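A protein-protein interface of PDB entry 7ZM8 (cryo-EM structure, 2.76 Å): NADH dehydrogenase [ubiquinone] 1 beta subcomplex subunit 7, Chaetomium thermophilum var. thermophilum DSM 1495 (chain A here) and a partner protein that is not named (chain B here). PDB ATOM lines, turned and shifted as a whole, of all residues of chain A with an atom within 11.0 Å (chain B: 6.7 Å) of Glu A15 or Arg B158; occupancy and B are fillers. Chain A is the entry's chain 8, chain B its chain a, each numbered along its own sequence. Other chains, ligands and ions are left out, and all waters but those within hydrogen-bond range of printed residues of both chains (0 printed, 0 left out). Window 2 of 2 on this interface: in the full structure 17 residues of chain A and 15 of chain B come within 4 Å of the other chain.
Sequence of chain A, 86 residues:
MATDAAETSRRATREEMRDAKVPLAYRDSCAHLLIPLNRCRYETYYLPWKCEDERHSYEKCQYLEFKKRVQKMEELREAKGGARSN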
ATOM      1  N   ARG A  11       7.041  -4.717 -21.416  1.00  0.00           N
ATOM      2  CA  ARG A  11       6.688  -3.557 -20.554  1.00  0.00           C
ATOM      3  C   ARG A  11       6.397  -2.337 -21.428  1.00  0.00           C
ATOM      4  O   ARG A  11       7.035  -2.210 -22.485  1.00  0.00           O
ATOM      5  CB  ARG A  11       7.844  -3.249 -19.603  1.00  0.00           C
ATOM      6  CG  ARG A  11       8.231  -4.405 -18.693  1.00  0.00           C
ATOM      7  CD  ARG A  11       9.377  -4.009 -17.782  1.00  0.00           C
ATOM      8  NE  ARG A  11       9.081  -2.778 -17.064  1.00  0.00           N
ATOM      9  CZ  ARG A  11       9.923  -2.167 -16.240  1.00  0.00           C
ATOM     10  NH1 ARG A  11       9.560  -1.050 -15.632  1.00  0.00           N
ATOM     11  NH2 ARG A  11      11.123  -2.671 -16.026  1.00  0.00           N
ATOM     12  N   ALA A  12       5.517  -1.440 -20.976  1.00  0.00           N
ATOM     13  CA  ALA A  12       5.234  -0.199 -21.735  1.00  0.00           C
ATOM     14  C   ALA A  12       6.345   0.823 -21.488  1.00  0.00           C
ATOM     15  O   ALA A  12       6.815   0.918 -20.338  1.00  0.00           O
ATOM     16  CB  ALA A  12       3.889   0.354 -21.355  1.00  0.00           C
ATOM     17  N   THR A  13       6.755   1.551 -22.532  1.00  0.00           N
ATOM     18  CA  THR A  13       7.809   2.592 -22.401  1.00  0.00           C
ATOM     19  C   THR A  13       7.255   3.796 -21.645  1.00  0.00           C
ATOM     20  O   THR A  13       6.048   4.025 -21.725  1.00  0.00           O
ATOM     21  CB  THR A  13       8.324   3.022 -23.780  1.00  0.00           C
ATOM     22  OG1 THR A  13       7.429   3.985 -24.335  1.00  0.00           O
ATOM     23  CG2 THR A  13       8.485   1.859 -24.733  1.00  0.00           C
ATOM     24  N   ARG A  14       8.119   4.534 -20.951  1.00  0.00           N
ATOM     25  CA  ARG A  14       7.678   5.747 -20.214  1.00  0.00           C
ATOM     26  C   ARG A  14       7.041   6.747 -21.184  1.00  0.00           C
ATOM     27  O   ARG A  14       6.162   7.495 -20.733  1.00  0.00           O
ATOM     28  CB  ARG A  14       8.803   6.312 -19.342  1.00  0.00           C
ATOM     29  CG  ARG A  14      10.130   6.514 -20.057  1.00  0.00           C
ATOM     30  CD  ARG A  14      11.201   6.779 -19.019  1.00  0.00           C
ATOM     31  NE  ARG A  14      10.748   7.757 -18.039  1.00  0.00           N
ATOM     32  CZ  ARG A  14      11.411   8.082 -16.936  1.00  0.00           C
ATOM     33  NH1 ARG A  14      10.914   8.985 -16.109  1.00  0.00           N
ATOM     34  NH2 ARG A  14      12.564   7.500 -16.660  1.00  0.00           N
ATOM     35  N   GLU A  15       7.456   6.759 -22.455  1.00  0.00           N
ATOM     36  CA  GLU A  15       6.787   7.622 -23.460  1.00  0.00           C
ATOM     37  C   GLU A  15       5.393   7.090 -23.765  1.00  0.00           C
ATOM     38  O   GLU A  15       4.505   7.910 -23.969  1.00  0.00           O
ATOM     39  CB  GLU A  15       7.585   7.614 -24.757  1.00  0.00           C
ATOM     40  CG  GLU A  15       9.077   7.795 -24.544  1.00  0.00           C
ATOM     41  CD  GLU A  15       9.481   9.097 -23.874  1.00  0.00           C
ATOM     42  OE1 GLU A  15       8.919  10.150 -24.237  1.00  0.00           O
ATOM     43  OE2 GLU A  15      10.351   9.053 -22.983  1.00  0.00           O
ATOM     44  N   GLU A  16       5.236   5.774 -23.887  1.00  0.00           N
ATOM     45  CA  GLU A  16       3.931   5.132 -24.170  1.00  0.00           C
ATOM     46  C   GLU A  16       2.989   5.331 -22.994  1.00  0.00           C
ATOM     47  O   GLU A  16       1.811   5.614 -23.238  1.00  0.00           O
ATOM     48  CB  GLU A  16       4.192   3.660 -24.470  1.00  0.00           C
ATOM     49  CG  GLU A  16       2.948   2.842 -24.755  1.00  0.00           C
ATOM     50  CD  GLU A  16       3.253   1.392 -25.085  1.00  0.00           C
ATOM     51  OE1 GLU A  16       4.450   1.042 -25.137  1.00  0.00           O
ATOM     52  OE2 GLU A  16       2.298   0.617 -25.287  1.00  0.00           O
ATOM     53  N   MET A  17       3.489   5.178 -21.768  1.00  0.00           N
ATOM     54  CA  MET A  17       2.665   5.448 -20.560  1.00  0.00           C
ATOM     55  C   MET A  17       2.302   6.934 -20.530  1.00  0.00           C
ATOM     56  O   MET A  17       1.175   7.248 -20.133  1.00  0.00           O
ATOM     57  CB  MET A  17       3.423   5.044 -19.298  1.00  0.00           C
ATOM     58  CG  MET A  17       3.916   3.615 -19.353  1.00  0.00           C
ATOM     59  SD  MET A  17       4.626   3.001 -17.810  1.00  0.00           S
ATOM     60  CE  MET A  17       5.981   4.143 -17.566  1.00  0.00           C
ATOM     61  N   ARG A  18       3.225   7.812 -20.932  1.00  0.00           N
ATOM     62  CA  ARG A  18       2.939   9.267 -21.020  1.00  0.00           C
ATOM     63  C   ARG A  18       1.931   9.511 -22.125  1.00  0.00           C
ATOM     64  O   ARG A  18       1.020  10.322 -21.926  1.00  0.00           O
ATOM     65  CB  ARG A  18       4.214  10.032 -21.376  1.00  0.00           C
ATOM     66  CG  ARG A  18       4.017  11.367 -22.074  1.00  0.00           C
ATOM     67  CD  ARG A  18       5.374  11.856 -22.536  1.00  0.00           C
ATOM     68  NE  ARG A  18       5.944  11.094 -23.635  1.00  0.00           N
ATOM     69  CZ  ARG A  18       5.963  11.506 -24.897  1.00  0.00           C
ATOM     70  NH1 ARG A  18       6.503  10.748 -25.835  1.00  0.00           N
ATOM     71  NH2 ARG A  18       5.445  12.679 -25.217  1.00  0.00           N
ATOM     72  N   ASP A  19       2.056   8.788 -23.228  1.00  0.00           N
ATOM     73  CA  ASP A  19       1.179   9.106 -24.343  1.00  0.00           C
ATOM     74  C   ASP A  19      -0.209   8.506 -24.172  1.00  0.00           C
ATOM     75  O   ASP A  19      -1.147   8.939 -24.848  1.00  0.00           O
ATOM     76  CB  ASP A  19       1.806   8.626 -25.649  1.00  0.00           C
ATOM     77  CG  ASP A  19       2.704   9.672 -26.280  1.00  0.00           C
ATOM     78  OD1 ASP A  19       3.094  10.627 -25.577  1.00  0.00           O
ATOM     79  OD2 ASP A  19       3.021   9.536 -27.481  1.00  0.00           O
ATOM     80  N   ALA A  20      -0.360   7.527 -23.288  1.00  0.00           N
ATOM     81  CA  ALA A  20      -1.652   6.940 -22.981  1.00  0.00           C
ATOM     82  C   ALA A  20      -2.229   7.438 -21.667  1.00  0.00           C
ATOM     83  O   ALA A  20      -3.192   6.847 -21.171  1.00  0.00           O
ATOM     84  CB  ALA A  20      -1.544   5.421 -22.947  1.00  0.00           C
ATOM     85  N   LYS A  21      -1.652   8.494 -21.088  1.00  0.00           N
ATOM     86  CA  LYS A  21      -2.211   9.171 -19.920  1.00  0.00           C
ATOM     87  C   LYS A  21      -2.444   8.207 -18.760  1.00  0.00           C
ATOM     88  O   LYS A  21      -3.485   8.238 -18.106  1.00  0.00           O
ATOM     89  CB  LYS A  21      -3.505   9.899 -20.288  1.00  0.00           C
ATOM     90  CG  LYS A  21      -3.317  11.145 -21.149  1.00  0.00           C
ATOM     91  CD  LYS A  21      -3.324  12.416 -20.316  1.00  0.00           C
ATOM     92  CE  LYS A  21      -4.565  12.483 -19.443  1.00  0.00           C
ATOM     93  NZ  LYS A  21      -4.647  13.747 -18.661  1.00  0.00           N
ATOM     94  N   VAL A  22      -1.481   7.328 -18.514  1.00  0.00           N
ATOM     95  CA  VAL A  22      -1.567   6.437 -17.350  1.00  0.00           C
ATOM     96  C   VAL A  22      -1.359   7.251 -16.080  1.00  0.00           C
ATOM     97  O   VAL A  22      -0.522   8.169 -16.073  1.00  0.00           O
ATOM     98  CB  VAL A  22      -0.530   5.318 -17.458  1.00  0.00           C
ATOM     99  CG1 VAL A  22      -0.829   4.221 -16.455  1.00  0.00           C
ATOM    100  CG2 VAL A  22      -0.499   4.761 -18.853  1.00  0.00           C
ATOM    101  N   LEU A  24       0.234   8.332 -12.631  1.00  0.00           N
ATOM    102  CA  LEU A  24       1.655   8.212 -12.308  1.00  0.00           C
ATOM    103  C   LEU A  24       1.946   7.048 -11.379  1.00  0.00           C
ATOM    104  O   LEU A  24       2.937   6.335 -11.572  1.00  0.00           O
ATOM    105  CB  LEU A  24       2.189   9.512 -11.707  1.00  0.00           C
ATOM    106  CG  LEU A  24       2.622  10.611 -12.669  1.00  0.00           C
ATOM    107  CD1 LEU A  24       3.785  10.062 -13.434  1.00  0.00           C
ATOM    108  CD2 LEU A  24       1.574  10.996 -13.626  1.00  0.00           C
ATOM    109  N   ARG A  27       2.488   3.765 -13.286  1.00  0.00           N
ATOM    110  CA  ARG A  27       3.473   3.665 -14.358  1.00  0.00           C
ATOM    111  C   ARG A  27       4.569   2.681 -13.987  1.00  0.00           C
ATOM    112  O   ARG A  27       5.759   2.960 -14.064  1.00  0.00           O
ATOM    113  CB  ARG A  27       4.035   5.044 -14.663  1.00  0.00           C
ATOM    114  CG  ARG A  27       2.946   6.033 -14.959  1.00  0.00           C
ATOM    115  CD  ARG A  27       3.353   7.065 -15.954  1.00  0.00           C
ATOM    116  NE  ARG A  27       2.218   7.921 -16.249  1.00  0.00           N
ATOM    117  CZ  ARG A  27       2.265   8.971 -17.051  1.00  0.00           C
ATOM    118  NH1 ARG A  27       3.403   9.312 -17.627  1.00  0.00           N
ATOM    119  NH2 ARG A  27       1.174   9.686 -17.258  1.00  0.00           N
ATOM    120  N   ASP A  28       4.135   1.506 -13.559  1.00  0.00           N
ATOM    121  CA  ASP A  28       4.997   0.427 -13.130  1.00  0.00           C
ATOM    122  C   ASP A  28       5.068  -0.642 -14.218  1.00  0.00           C
ATOM    123  O   ASP A  28       4.570  -0.459 -15.328  1.00  0.00           O
ATOM    124  CB  ASP A  28       4.516  -0.098 -11.773  1.00  0.00           C
ATOM    125  CG  ASP A  28       3.115  -0.684 -11.820  1.00  0.00           C
ATOM    126  OD1 ASP A  28       2.470  -0.660 -12.889  1.00  0.00           O
ATOM    127  OD2 ASP A  28       2.648  -1.162 -10.765  1.00  0.00           O
ATOM    128  N   ALA A  31       2.009  -1.819 -16.345  1.00  0.00           N
ATOM    129  CA  ALA A  31       1.173  -0.802 -16.964  1.00  0.00           C
ATOM    130  C   ALA A  31       0.814  -1.125 -18.406  1.00  0.00           C
ATOM    131  O   ALA A  31      -0.018  -0.429 -18.989  1.00  0.00           O
ATOM    132  CB  ALA A  31       1.866   0.561 -16.898  1.00  0.00           C
ATOM    133  N   ILE A  35      -3.030  -0.334 -20.058  1.00  0.00           N
ATOM    134  CA  ILE A  35      -3.364   0.387 -21.285  1.00  0.00           C
ATOM    135  C   ILE A  35      -4.668  -0.116 -21.894  1.00  0.00           C
ATOM    136  O   ILE A  35      -5.572   0.704 -22.121  1.00  0.00           O
ATOM    137  CB  ILE A  35      -2.186   0.329 -22.273  1.00  0.00           C
ATOM    138  CG1 ILE A  35      -0.935   0.938 -21.655  1.00  0.00           C
ATOM    139  CG2 ILE A  35      -2.540   1.055 -23.561  1.00  0.00           C
ATOM    140  CD1 ILE A  35      -1.093   2.359 -21.295  1.00  0.00           C
ATOM    141  N   GLY B 154      13.632   4.499 -13.044  1.00  0.00           N
ATOM    142  CA  GLY B 154      14.180   5.835 -13.036  1.00  0.00           C
ATOM    143  C   GLY B 154      13.582   6.766 -12.008  1.00  0.00           C
ATOM    144  O   GLY B 154      13.889   7.963 -12.030  1.00  0.00           O
ATOM    145  N   GLY B 155      12.744   6.265 -11.107  1.00  0.00           N
ATOM    146  CA  GLY B 155      12.079   7.111 -10.147  1.00  0.00           C
ATOM    147  C   GLY B 155      11.035   8.028 -10.734  1.00  0.00           C
ATOM    148  O   GLY B 155      10.501   8.869 -10.006  1.00  0.00           O
ATOM    149  N   LEU B 156      10.733   7.897 -12.028  1.00  0.00           N
ATOM    150  CA  LEU B 156       9.731   8.723 -12.699  1.00  0.00           C
ATOM    151  C   LEU B 156      10.068  10.202 -12.570  1.00  0.00           C
ATOM    152  O   LEU B 156       9.184  11.060 -12.560  1.00  0.00           O
ATOM    153  CB  LEU B 156       8.329   8.436 -12.160  1.00  0.00           C
ATOM    154  CG  LEU B 156       7.476   7.378 -12.851  1.00  0.00           C
ATOM    155  CD1 LEU B 156       8.233   6.078 -12.970  1.00  0.00           C
ATOM    156  CD2 LEU B 156       6.199   7.171 -12.076  1.00  0.00           C
ATOM    157  N   GLU B 157      11.365  10.502 -12.479  1.00  0.00           N
ATOM    158  CA  GLU B 157      11.790  11.846 -12.109  1.00  0.00           C
ATOM    159  C   GLU B 157      11.341  12.879 -13.136  1.00  0.00           C
ATOM    160  O   GLU B 157      11.032  14.020 -12.781  1.00  0.00           O
ATOM    161  CB  GLU B 157      13.307  11.880 -11.921  1.00  0.00           C
ATOM    162  CG  GLU B 157      14.097  11.325 -13.093  1.00  0.00           C
ATOM    163  CD  GLU B 157      14.516  12.408 -14.067  1.00  0.00           C
ATOM    164  OE1 GLU B 157      14.531  13.589 -13.664  1.00  0.00           O
ATOM    165  OE2 GLU B 157      14.820  12.080 -15.233  1.00  0.00           O
ATOM    166  N   ARG B 158      11.292  12.501 -14.415  1.00  0.00           N
ATOM    167  CA  ARG B 158      10.796  13.427 -15.427  1.00  0.00           C
ATOM    168  C   ARG B 158       9.306  13.675 -15.252  1.00  0.00           C
ATOM    169  O   ARG B 158       8.853  14.823 -15.216  1.00  0.00           O
ATOM    170  CB  ARG B 158      11.086  12.891 -16.827  1.00  0.00           C
ATOM    171  CG  ARG B 158      10.571  13.802 -17.929  1.00  0.00           C
ATOM    172  CD  ARG B 158      11.105  13.425 -19.299  1.00  0.00           C
ATOM    173  NE  ARG B 158      10.816  12.041 -19.655  1.00  0.00           N
ATOM    174  CZ  ARG B 158      11.725  11.185 -20.113  1.00  0.00           C
ATOM    175  NH1 ARG B 158      11.376   9.944 -20.415  1.00  0.00           N
ATOM    176  NH2 ARG B 158      12.983  11.575 -20.272  1.00  0.00           N
ATOM    177  N   GLU B 159       8.531  12.603 -15.114  1.00  0.00           N
ATOM    178  CA  GLU B 159       7.085  12.699 -15.019  1.00  0.00           C
ATOM    179  C   GLU B 159       6.607  13.334 -13.724  1.00  0.00           C
ATOM    180  O   GLU B 159       5.429  13.692 -13.629  1.00  0.00           O
ATOM    181  CB  GLU B 159       6.483  11.310 -15.175  1.00  0.00           C
ATOM    182  CG  GLU B 159       6.137  10.954 -16.598  1.00  0.00           C
ATOM    183  CD  GLU B 159       7.349  10.876 -17.501  1.00  0.00           C
ATOM    184  OE1 GLU B 159       8.475  10.759 -16.981  1.00  0.00           O
ATOM    185  OE2 GLU B 159       7.175  10.944 -18.737  1.00  0.00           O
ATOM    186  N   LEU B 160       7.471  13.484 -12.729  1.00  0.00           N
ATOM    187  CA  LEU B 160       7.079  14.085 -11.466  1.00  0.00           C
ATOM    188  C   LEU B 160       7.649  15.482 -11.280  1.00  0.00           C
ATOM    189  O   LEU B 160       7.522  16.050 -10.195  1.00  0.00           O
ATOM    190  CB  LEU B 160       7.488  13.180 -10.305  1.00  0.00           C
ATOM    191  CG  LEU B 160       6.556  11.979 -10.140  1.00  0.00           C
ATOM    192  CD1 LEU B 160       7.275  10.785  -9.541  1.00  0.00           C
ATOM    193  CD2 LEU B 160       5.354  12.366  -9.301  1.00  0.00           C
ATOM    194  N   GLY B 161       8.263  16.054 -12.309  1.00  0.00           N
ATOM    195  CA  GLY B 161       8.715  17.433 -12.263  1.00  0.00           C
ATOM    196  C   GLY B 161      10.204  17.646 -12.443  1.00  0.00           C
ATOM    197  O   GLY B 161      10.654  18.796 -12.367  1.00  0.00           O
ATOM    198  N   GLY B 162      10.999  16.616 -12.681  1.00  0.00           N
ATOM    199  CA  GLY B 162      12.415  16.793 -12.906  1.00  0.00           C
ATOM    200  C   GLY B 162      13.227  16.572 -11.649  1.00  0.00           C
ATOM    201  O   GLY B 162      12.736  16.119 -10.612  1.00  0.00           O
ATOM    202  N   ALA B 163      14.517  16.896 -11.762  1.00  0.00           N
ATOM    203  CA  ALA B 163      15.411  16.799 -10.617  1.00  0.00           C
ATOM    204  C   ALA B 163      15.010  17.746  -9.501  1.00  0.00           C
ATOM    205  O   ALA B 163      15.310  17.477  -8.333  1.00  0.00           O
ATOM    206  CB  ALA B 163      16.849  17.081 -11.050  1.00  0.00           C
ATOM    207  N   ARG B 167      10.557  12.588  -6.244  1.00  0.00           N
ATOM    208  CA  ARG B 167      10.248  11.461  -7.109  1.00  0.00           C
ATOM    209  C   ARG B 167       9.962  10.221  -6.268  1.00  0.00           C
ATOM    210  O   ARG B 167       9.949  10.264  -5.036  1.00  0.00           O
ATOM    211  CB  ARG B 167      11.395  11.197  -8.081  1.00  0.00           C
ATOM    212  CG  ARG B 167      12.727  10.971  -7.406  1.00  0.00           C
ATOM    213  CD  ARG B 167      13.503   9.876  -8.107  1.00  0.00           C
ATOM    214  NE  ARG B 167      14.826   9.683  -7.529  1.00  0.00           N
ATOM    215  CZ  ARG B 167      15.071   8.926  -6.466  1.00  0.00           C
ATOM    216  NH1 ARG B 167      14.080   8.288  -5.863  1.00  0.00           N
ATOM    217  NH2 ARG B 167      16.308   8.808  -6.007  1.00  0.00           N
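OE2 of Glu A15 is in salt-bridge range of NH1 of Arg B158, at 2.9 Å.
OE1 of Glu B159 is in salt-bridge range of NH1 of Arg A14 (3.1 Å).
The guanidinium group of Arg A14 sits close to the guanidinium group of Arg B158, 3.3 Å away.
The backbone NH (N) of Gly B162 lies within hydrogen-bond range of the backbone carbonyl oxygen (O) of Glu B157.
OE1 of Glu B159 lies within salt-bridge range of NE of Arg B158 (3.8 Å).
The side-chain hydroxyl (OG1) of Thr A13 lies close to the backbone NH (N) of Glu A15 (3.4 Å).
The side-chain carboxylate (OE1) of Glu A15 lies within salt-bridge range of the guanidinium group (NH1) of Arg A18, 3.0 Å away.
O of Val A22 sits at hydrogen-bond distance from NH2 of Arg A27.
NH1 of Arg A14 touches CA of Leu B156, at 3.6 Å.
NH1 of Arg A14 touches N of Glu B157, at 3.96 Å.
Leu A24 touches Leu B156.
Leu A24 touches Glu B159.
CB of Arg A27 touches CD2 of Leu B156, 3.99 Å away.
Arg A27 touches Glu B159 (NH1 to CG, 3.4 Å).
Hydrophobic or aromatic side chains of chain A within 4 Å of the printed part of chain B: Leu A24.
Along chain A the printed residues that touch a printed residue of chain B span positions 14 to 27.
Of the 11 printed residues of chain B, 4 touch a printed residue of chain A.
Hydrophobic or aromatic side chains of chain B that line the printed part of chain A: Leu B156.
Among the printed residues, Asp or Glu carboxylates within 4 Å of a Lys or Arg side-chain nitrogen of the other chain: Arg A14 with Glu B159 (3.1 Å) and Glu A15 with Arg B158 (2.9 Å).
Glu A15 touches one residue of chain B.
Printed residues of chain A within 4 Å of Arg B158: Arg A14 and Glu A15.
Glu B157 touches just one residue of chain A: Arg A14.
No residue of chain A comes within 4 Å of Gly B161.
Printed residues of chain A within 4 Å of Leu B156: Arg A14 (3.6 Å), Leu A24 (3.4 Å) and Arg A27 (3.99 Å).
Printed residues of chain B within 4 Å of Arg A27: Leu B156 and Glu B159.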
